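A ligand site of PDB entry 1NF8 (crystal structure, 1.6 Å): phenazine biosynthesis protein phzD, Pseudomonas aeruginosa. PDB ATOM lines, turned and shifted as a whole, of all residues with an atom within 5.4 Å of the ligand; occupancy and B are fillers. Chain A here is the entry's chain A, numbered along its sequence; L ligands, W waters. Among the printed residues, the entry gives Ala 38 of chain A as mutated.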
ATOM      1  N   SER A   2      -5.532  36.712  18.410  1.00  0.00           N
ATOM      2  CA  SER A   2      -4.814  35.509  18.789  1.00  0.00           C
ATOM      3  C   SER A   2      -4.773  34.477  17.676  1.00  0.00           C
ATOM      4  O   SER A   2      -3.842  33.672  17.615  1.00  0.00           O
ATOM      5  CB  SER A   2      -5.497  34.882  20.021  1.00  0.00           C
ATOM      6  OG  SER A   2      -6.775  34.360  19.716  1.00  0.00           O
ATOM      7  N   ILE A   4      -6.770  32.145  17.593  1.00  0.00           N
ATOM      8  CA  ILE A   4      -7.361  30.938  18.197  1.00  0.00           C
ATOM      9  C   ILE A   4      -8.861  31.071  18.201  1.00  0.00           C
ATOM     10  O   ILE A   4      -9.431  32.037  18.695  1.00  0.00           O
ATOM     11  CB  ILE A   4      -6.779  30.747  19.603  1.00  0.00           C
ATOM     12  CG1 ILE A   4      -5.268  30.524  19.593  1.00  0.00           C
ATOM     13  CG2 ILE A   4      -7.507  29.640  20.344  1.00  0.00           C
ATOM     14  CD1 ILE A   4      -4.613  30.599  20.958  1.00  0.00           C
ATOM     15  N   HIS A  37       3.697  20.068  26.865  1.00  0.00           N
ATOM     16  CA  HIS A  37       3.746  20.973  25.726  1.00  0.00           C
ATOM     17  C   HIS A  37       2.788  22.149  25.837  1.00  0.00           C
ATOM     18  O   HIS A  37       1.570  21.975  25.659  1.00  0.00           O
ATOM     19  CB  HIS A  37       3.421  20.171  24.451  1.00  0.00           C
ATOM     20  CG  HIS A  37       3.537  21.024  23.218  1.00  0.00           C
ATOM     21  ND1 HIS A  37       2.569  21.907  22.828  1.00  0.00           N
ATOM     22  CD2 HIS A  37       4.531  21.143  22.291  1.00  0.00           C
ATOM     23  CE1 HIS A  37       2.956  22.525  21.713  1.00  0.00           C
ATOM     24  NE2 HIS A  37       4.152  22.094  21.368  1.00  0.00           N
ATOM     25  N   ALA A  38       3.347  23.324  26.054  1.00  0.00           N
ATOM     26  CA  ALA A  38       2.694  24.615  25.987  1.00  0.00           C
ATOM     27  C   ALA A  38       1.503  24.687  26.918  1.00  0.00           C
ATOM     28  O   ALA A  38       0.481  25.284  26.537  1.00  0.00           O
ATOM     29  CB  ALA A  38       2.236  24.963  24.566  1.00  0.00           C
ATOM     30  N   TYR A  42      -2.051  31.288  28.950  1.00  0.00           N
ATOM     31  CA  TYR A  42      -2.614  31.881  27.719  1.00  0.00           C
ATOM     32  C   TYR A  42      -3.232  30.845  26.783  1.00  0.00           C
ATOM     33  O   TYR A  42      -4.250  31.090  26.147  1.00  0.00           O
ATOM     34  CB  TYR A  42      -1.504  32.612  26.979  1.00  0.00           C
ATOM     35  CG  TYR A  42      -1.782  33.222  25.630  1.00  0.00           C
ATOM     36  CD1 TYR A  42      -1.601  32.494  24.460  1.00  0.00           C
ATOM     37  CD2 TYR A  42      -2.190  34.533  25.494  1.00  0.00           C
ATOM     38  CE1 TYR A  42      -1.841  33.043  23.217  1.00  0.00           C
ATOM     39  CE2 TYR A  42      -2.434  35.089  24.262  1.00  0.00           C
ATOM     40  CZ  TYR A  42      -2.264  34.344  23.118  1.00  0.00           C
ATOM     41  OH  TYR A  42      -2.488  34.878  21.863  1.00  0.00           O
ATOM     42  N   PHE A  43      -2.570  29.703  26.655  1.00  0.00           N
ATOM     43  CA  PHE A  43      -3.091  28.704  25.707  1.00  0.00           C
ATOM     44  C   PHE A  43      -4.261  27.906  26.263  1.00  0.00           C
ATOM     45  O   PHE A  43      -4.991  27.292  25.449  1.00  0.00           O
ATOM     46  CB  PHE A  43      -1.994  27.755  25.258  1.00  0.00           C
ATOM     47  CG  PHE A  43      -0.919  28.404  24.395  1.00  0.00           C
ATOM     48  CD1 PHE A  43      -1.247  29.092  23.251  1.00  0.00           C
ATOM     49  CD2 PHE A  43       0.419  28.288  24.735  1.00  0.00           C
ATOM     50  CE1 PHE A  43      -0.287  29.690  22.467  1.00  0.00           C
ATOM     51  CE2 PHE A  43       1.391  28.905  23.977  1.00  0.00           C
ATOM     52  CZ  PHE A  43       1.051  29.601  22.833  1.00  0.00           C
ATOM     53  N   GLN A  78       6.700  29.450  25.655  1.00  0.00           N
ATOM     54  CA  GLN A  78       6.959  30.686  24.956  1.00  0.00           C
ATOM     55  C   GLN A  78       7.347  31.739  26.011  1.00  0.00           C
ATOM     56  O   GLN A  78       6.838  31.768  27.137  1.00  0.00           O
ATOM     57  CB  GLN A  78       5.801  31.230  24.137  1.00  0.00           C
ATOM     58  CG  GLN A  78       5.379  30.392  22.936  1.00  0.00           C
ATOM     59  CD  GLN A  78       4.443  31.117  21.984  1.00  0.00           C
ATOM     60  OE1 GLN A  78       3.914  32.205  22.251  1.00  0.00           O
ATOM     61  NE2 GLN A  78       4.246  30.506  20.813  1.00  0.00           N
ATOM     62  N   ARG A  87       9.054  36.866  16.465  1.00  0.00           N
ATOM     63  CA  ARG A  87       7.708  36.409  16.112  1.00  0.00           C
ATOM     64  C   ARG A  87       7.626  35.904  14.668  1.00  0.00           C
ATOM     65  O   ARG A  87       6.935  34.919  14.371  1.00  0.00           O
ATOM     66  CB  ARG A  87       6.739  37.553  16.338  1.00  0.00           C
ATOM     67  CG  ARG A  87       5.267  37.238  16.318  1.00  0.00           C
ATOM     68  CD  ARG A  87       4.868  36.319  17.464  1.00  0.00           C
ATOM     69  NE  ARG A  87       3.431  35.993  17.435  1.00  0.00           N
ATOM     70  CZ  ARG A  87       2.898  34.986  18.116  1.00  0.00           C
ATOM     71  NH1 ARG A  87       3.649  34.205  18.881  1.00  0.00           N
ATOM     72  NH2 ARG A  87       1.596  34.743  18.038  1.00  0.00           N
ATOM     73  N   LEU A  90       4.739  33.902  12.586  1.00  0.00           N
ATOM     74  CA  LEU A  90       3.615  33.548  13.481  1.00  0.00           C
ATOM     75  C   LEU A  90       2.585  34.675  13.471  1.00  0.00           C
ATOM     76  O   LEU A  90       1.394  34.448  13.706  1.00  0.00           O
ATOM     77  CB  LEU A  90       4.068  33.352  14.922  1.00  0.00           C
ATOM     78  CG  LEU A  90       5.006  32.181  15.180  1.00  0.00           C
ATOM     79  CD1 LEU A  90       5.462  32.110  16.626  1.00  0.00           C
ATOM     80  CD2 LEU A  90       4.286  30.884  14.776  1.00  0.00           C
ATOM     81  N   TRP A  94      -1.329  34.302  13.962  1.00  0.00           N
ATOM     82  CA  TRP A  94      -1.578  34.276  15.416  1.00  0.00           C
ATOM     83  C   TRP A  94      -1.347  35.601  16.117  1.00  0.00           C
ATOM     84  O   TRP A  94      -1.348  35.681  17.364  1.00  0.00           O
ATOM     85  CB  TRP A  94      -0.697  33.197  16.034  1.00  0.00           C
ATOM     86  CG  TRP A  94      -0.674  31.878  15.354  1.00  0.00           C
ATOM     87  CD1 TRP A  94       0.364  31.359  14.624  1.00  0.00           C
ATOM     88  CD2 TRP A  94      -1.704  30.868  15.329  1.00  0.00           C
ATOM     89  NE1 TRP A  94       0.031  30.093  14.159  1.00  0.00           N
ATOM     90  CE2 TRP A  94      -1.231  29.777  14.573  1.00  0.00           C
ATOM     91  CE3 TRP A  94      -2.974  30.779  15.870  1.00  0.00           C
ATOM     92  CZ2 TRP A  94      -1.969  28.624  14.339  1.00  0.00           C
ATOM     93  CZ3 TRP A  94      -3.694  29.640  15.641  1.00  0.00           C
ATOM     94  CH2 TRP A  94      -3.217  28.581  14.881  1.00  0.00           C
ATOM     95  N   GLY A  97       0.988  37.598  19.765  1.00  0.00           N
ATOM     96  CA  GLY A  97       1.037  36.518  20.726  1.00  0.00           C
ATOM     97  C   GLY A  97       1.053  36.945  22.168  1.00  0.00           C
ATOM     98  O   GLY A  97       0.906  38.134  22.510  1.00  0.00           O
ATOM     99  N   MET A  98       1.219  35.987  23.074  1.00  0.00           N
ATOM    100  CA  MET A  98       1.062  36.282  24.490  1.00  0.00           C
ATOM    101  C   MET A  98       2.128  37.263  24.975  1.00  0.00           C
ATOM    102  O   MET A  98       3.173  37.489  24.352  1.00  0.00           O
ATOM    103  CB  MET A  98       1.134  34.986  25.277  1.00  0.00           C
ATOM    104  CG  MET A  98       2.567  34.556  25.515  1.00  0.00           C
ATOM    105  SD  MET A  98       2.739  33.045  26.487  1.00  0.00           S
ATOM    106  CE  MET A  98       2.179  31.798  25.342  1.00  0.00           C
ATOM    107  N   LYS A 122       9.783  27.623  23.777  1.00  0.00           N
ATOM    108  CA  LYS A 122       8.998  27.365  22.565  1.00  0.00           C
ATOM    109  C   LYS A 122       9.029  28.600  21.665  1.00  0.00           C
ATOM    110  O   LYS A 122       8.675  29.684  22.147  1.00  0.00           O
ATOM    111  CB  LYS A 122       7.547  27.028  22.892  1.00  0.00           C
ATOM    112  CG  LYS A 122       6.592  26.857  21.719  1.00  0.00           C
ATOM    113  CD  LYS A 122       5.259  26.332  22.279  1.00  0.00           C
ATOM    114  CE  LYS A 122       4.100  26.460  21.326  1.00  0.00           C
ATOM    115  NZ  LYS A 122       4.459  25.953  19.975  1.00  0.00           N
ATOM    116  N   ARG A 124       8.423  27.839  17.840  1.00  0.00           N
ATOM    117  CA  ARG A 124       7.606  27.477  16.707  1.00  0.00           C
ATOM    118  C   ARG A 124       6.820  26.200  17.008  1.00  0.00           C
ATOM    119  O   ARG A 124       6.823  25.726  18.145  1.00  0.00           O
ATOM    120  CB  ARG A 124       8.469  27.402  15.439  1.00  0.00           C
ATOM    121  CG  ARG A 124       9.037  28.757  15.036  1.00  0.00           C
ATOM    122  CD  ARG A 124       7.998  29.782  14.635  1.00  0.00           C
ATOM    123  NE  ARG A 124       8.621  30.986  14.034  1.00  0.00           N
ATOM    124  CZ  ARG A 124       9.121  32.021  14.679  1.00  0.00           C
ATOM    125  NH1 ARG A 124       9.092  32.030  16.001  1.00  0.00           N
ATOM    126  NH2 ARG A 124       9.664  33.071  14.069  1.00  0.00           N
ATOM    127  N   TYR A 125       6.133  25.669  16.010  1.00  0.00           N
ATOM    128  CA  TYR A 125       5.236  24.524  16.242  1.00  0.00           C
ATOM    129  C   TYR A 125       5.970  23.355  16.866  1.00  0.00           C
ATOM    130  O   TYR A 125       5.507  22.725  17.825  1.00  0.00           O
ATOM    131  CB  TYR A 125       4.518  24.067  14.947  1.00  0.00           C
ATOM    132  CG  TYR A 125       3.605  25.107  14.328  1.00  0.00           C
ATOM    133  CD1 TYR A 125       3.089  26.184  15.046  1.00  0.00           C
ATOM    134  CD2 TYR A 125       3.218  25.008  13.000  1.00  0.00           C
ATOM    135  CE1 TYR A 125       2.254  27.121  14.466  1.00  0.00           C
ATOM    136  CE2 TYR A 125       2.395  25.951  12.403  1.00  0.00           C
ATOM    137  CZ  TYR A 125       1.902  27.011  13.130  1.00  0.00           C
ATOM    138  OH  TYR A 125       1.073  27.933  12.528  1.00  0.00           O
ATOM    139  N   VAL A 150      -1.207  21.114  24.576  1.00  0.00           N
ATOM    140  CA  VAL A 150      -2.003  21.746  23.519  1.00  0.00           C
ATOM    141  C   VAL A 150      -1.141  22.416  22.471  1.00  0.00           C
ATOM    142  O   VAL A 150       0.025  22.772  22.792  1.00  0.00           O
ATOM    143  CB  VAL A 150      -2.909  22.825  24.151  1.00  0.00           C
ATOM    144  CG1 VAL A 150      -3.851  22.188  25.134  1.00  0.00           C
ATOM    145  CG2 VAL A 150      -2.061  23.898  24.833  1.00  0.00           C
ATOM    146  N   TYR A 151      -1.637  22.595  21.258  1.00  0.00           N
ATOM    147  CA  TYR A 151      -2.866  22.114  20.658  1.00  0.00           C
ATOM    148  C   TYR A 151      -2.577  20.835  19.884  1.00  0.00           C
ATOM    149  O   TYR A 151      -1.526  20.749  19.200  1.00  0.00           O
ATOM    150  CB  TYR A 151      -3.509  23.176  19.747  1.00  0.00           C
ATOM    151  CG  TYR A 151      -3.846  24.391  20.585  1.00  0.00           C
ATOM    152  CD1 TYR A 151      -4.870  24.410  21.515  1.00  0.00           C
ATOM    153  CD2 TYR A 151      -3.099  25.536  20.448  1.00  0.00           C
ATOM    154  CE1 TYR A 151      -5.117  25.571  22.250  1.00  0.00           C
ATOM    155  CE2 TYR A 151      -3.322  26.682  21.184  1.00  0.00           C
ATOM    156  CZ  TYR A 151      -4.354  26.701  22.102  1.00  0.00           C
ATOM    157  OH  TYR A 151      -4.585  27.833  22.844  1.00  0.00           O
ATOM    158  N   VAL A 154      -1.601  21.072  16.208  1.00  0.00           N
ATOM    159  CA  VAL A 154      -0.569  22.048  15.815  1.00  0.00           C
ATOM    160  C   VAL A 154       0.747  21.628  16.441  1.00  0.00           C
ATOM    161  O   VAL A 154       1.366  20.661  15.962  1.00  0.00           O
ATOM    162  CB  VAL A 154      -1.009  23.479  16.160  1.00  0.00           C
ATOM    163  CG1 VAL A 154       0.036  24.477  15.660  1.00  0.00           C
ATOM    164  CG2 VAL A 154      -2.393  23.750  15.579  1.00  0.00           C
ATOM    165  N   GLY A 155       1.232  22.275  17.509  1.00  0.00           N
ATOM    166  CA  GLY A 155       2.525  21.950  18.089  1.00  0.00           C
ATOM    167  C   GLY A 155       2.701  20.543  18.641  1.00  0.00           C
ATOM    168  O   GLY A 155       3.784  19.942  18.578  1.00  0.00           O
ATOM    169  N   VAL A 156       1.625  19.975  19.203  1.00  0.00           N
ATOM    170  CA  VAL A 156       1.745  18.613  19.716  1.00  0.00           C
ATOM    171  C   VAL A 156       2.055  17.652  18.576  1.00  0.00           C
ATOM    172  O   VAL A 156       3.004  16.860  18.643  1.00  0.00           O
ATOM    173  CB  VAL A 156       0.467  18.214  20.471  1.00  0.00           C
ATOM    174  CG1 VAL A 156       0.473  16.725  20.771  1.00  0.00           C
ATOM    175  CG2 VAL A 156       0.399  19.000  21.769  1.00  0.00           C
ATOM    176  N   PHE A 180      -8.641  22.597  19.140  1.00  0.00           N
ATOM    177  CA  PHE A 180      -9.638  23.581  18.725  1.00  0.00           C
ATOM    178  C   PHE A 180     -11.032  23.006  18.570  1.00  0.00           C
ATOM    179  O   PHE A 180     -12.034  23.737  18.597  1.00  0.00           O
ATOM    180  CB  PHE A 180      -9.263  24.197  17.362  1.00  0.00           C
ATOM    181  CG  PHE A 180      -8.034  25.097  17.399  1.00  0.00           C
ATOM    182  CD1 PHE A 180      -7.353  25.322  18.591  1.00  0.00           C
ATOM    183  CD2 PHE A 180      -7.572  25.689  16.236  1.00  0.00           C
ATOM    184  CE1 PHE A 180      -6.233  26.142  18.629  1.00  0.00           C
ATOM    185  CE2 PHE A 180      -6.460  26.509  16.264  1.00  0.00           C
ATOM    186  CZ  PHE A 180      -5.791  26.742  17.456  1.00  0.00           C
HETATM  187  C1  LIG L   1       1.106  31.675  19.115  1.00  0.00           C
HETATM  188  C2  LIG L   1       0.625  30.280  18.771  1.00  0.00           C
HETATM  189  O1  LIG L   1       0.371  32.632  19.424  1.00  0.00           O
HETATM  190  C3  LIG L   1       1.553  29.099  18.461  1.00  0.00           C
HETATM  191  O2  LIG L   1       2.353  31.778  19.077  1.00  0.00           O
HETATM  192  C4  LIG L   1       1.068  27.853  18.588  1.00  0.00           C
HETATM  193  O3  LIG L   1       2.339  29.420  17.396  1.00  0.00           O
HETATM  194  C5  LIG L   1      -0.358  27.681  18.221  1.00  0.00           C
HETATM  195  C6  LIG L   1      -1.247  28.752  18.309  1.00  0.00           C
HETATM  196  C7  LIG L   1      -0.828  30.050  18.647  1.00  0.00           C
HETATM  197  C8  LIG L   1       1.061  24.972  19.564  1.00  0.00           C
HETATM  198  O4  LIG L   1       0.197  24.069  19.458  1.00  0.00           O
HETATM  199  C9  LIG L   1       0.802  26.152  20.353  1.00  0.00           C
HETATM  200  O5  LIG L   1       2.076  25.043  18.826  1.00  0.00           O
HETATM  201  C10 LIG L   1       0.165  25.948  21.623  1.00  0.00           C
HETATM  202  O6  LIG L   1       1.158  27.396  19.934  1.00  0.00           O
HETATM  203  O   HOH W   1       5.139  28.701  18.476  1.00  0.00           O
HETATM  204  O   HOH W   2       1.587  33.434  21.923  1.00  0.00           O
HETATM  205  O   HOH W   3      -2.240  33.306  19.743  1.00  0.00           O
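An oxygen (O2) of the ligand lies within salt-bridge range of the guanidinium group (NH1) of Arg 87 (2.8 Å). An oxygen (O5) of the ligand lies within salt-bridge range of the side-chain amino group (NZ) of Lys 122 (2.8 Å). N of Gly 155 sits at hydrogen-bond distance from O4 of the ligand. The side-chain amide nitrogen (NE2) of Gln 78 sits at hydrogen-bond distance from an oxygen (O2) of the ligand. An oxygen (O4) of the ligand sits at hydrogen-bond distance from the backbone NH of Tyr 151 (3.0 Å).
NH2 of Arg 87 is in hydrogen-bond range of O of Trp 94 (3.2 Å). The guanidinium group of Arg 124 sits at hydrogen-bond distance from the backbone carbonyl oxygen of Arg 87 (3.3 Å). NZ of Lys 122 lies within hydrogen-bond range of O of Arg 124 (3.0 Å). The side-chain hydroxyl (OH) of Tyr 151 is in hydrogen-bond range of the backbone carbonyl oxygen (O) of Phe 43, at 2.7 Å. O of Tyr 151 is in hydrogen-bond range of N of Val 156 (3.2 Å). The backbone carbonyl oxygen (O) of Val 150 lies within hydrogen-bond range of a ring nitrogen (ND1) of His 37, 2.7 Å away. NE1 of Trp 94 is in hydrogen-bond range of OH of Tyr 125, at 2.9 Å.
Residues that only touch the ligand: Val 150, Trp 94, Val 154, Leu 90, Phe 43, Tyr 125, Ala 38 and His 37. 13 residues have an atom within 4 Å of the ligand: His 37, Ala 38, Phe 43, Gln 78, Arg 87, Leu 90, Trp 94, Lys 122, Tyr 125, Val 150, Tyr 151, Val 154 and Gly 155.
Water W3 lies within hydrogen-bond range of OH of Tyr 42 (2.7 Å), O of Ser 2 (2.7 Å), O1 of the ligand (2.7 Å) and O of Trp 94 (3.5 Å). Water W2 lies within hydrogen-bond range of the side-chain amide oxygen of Gln 78 (2.7 Å), the backbone NH of Met 98 (2.8 Å) and an oxygen (O1) of the ligand (2.9 Å). Water W1 lies within hydrogen-bond range of the side-chain amide nitrogen of Gln 78 (3.1 Å), an oxygen (O3) of the ligand (3.1 Å), the side-chain amino group of Lys 122 (3.2 Å) and the backbone carbonyl oxygen of Arg 124 (3.4 Å).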
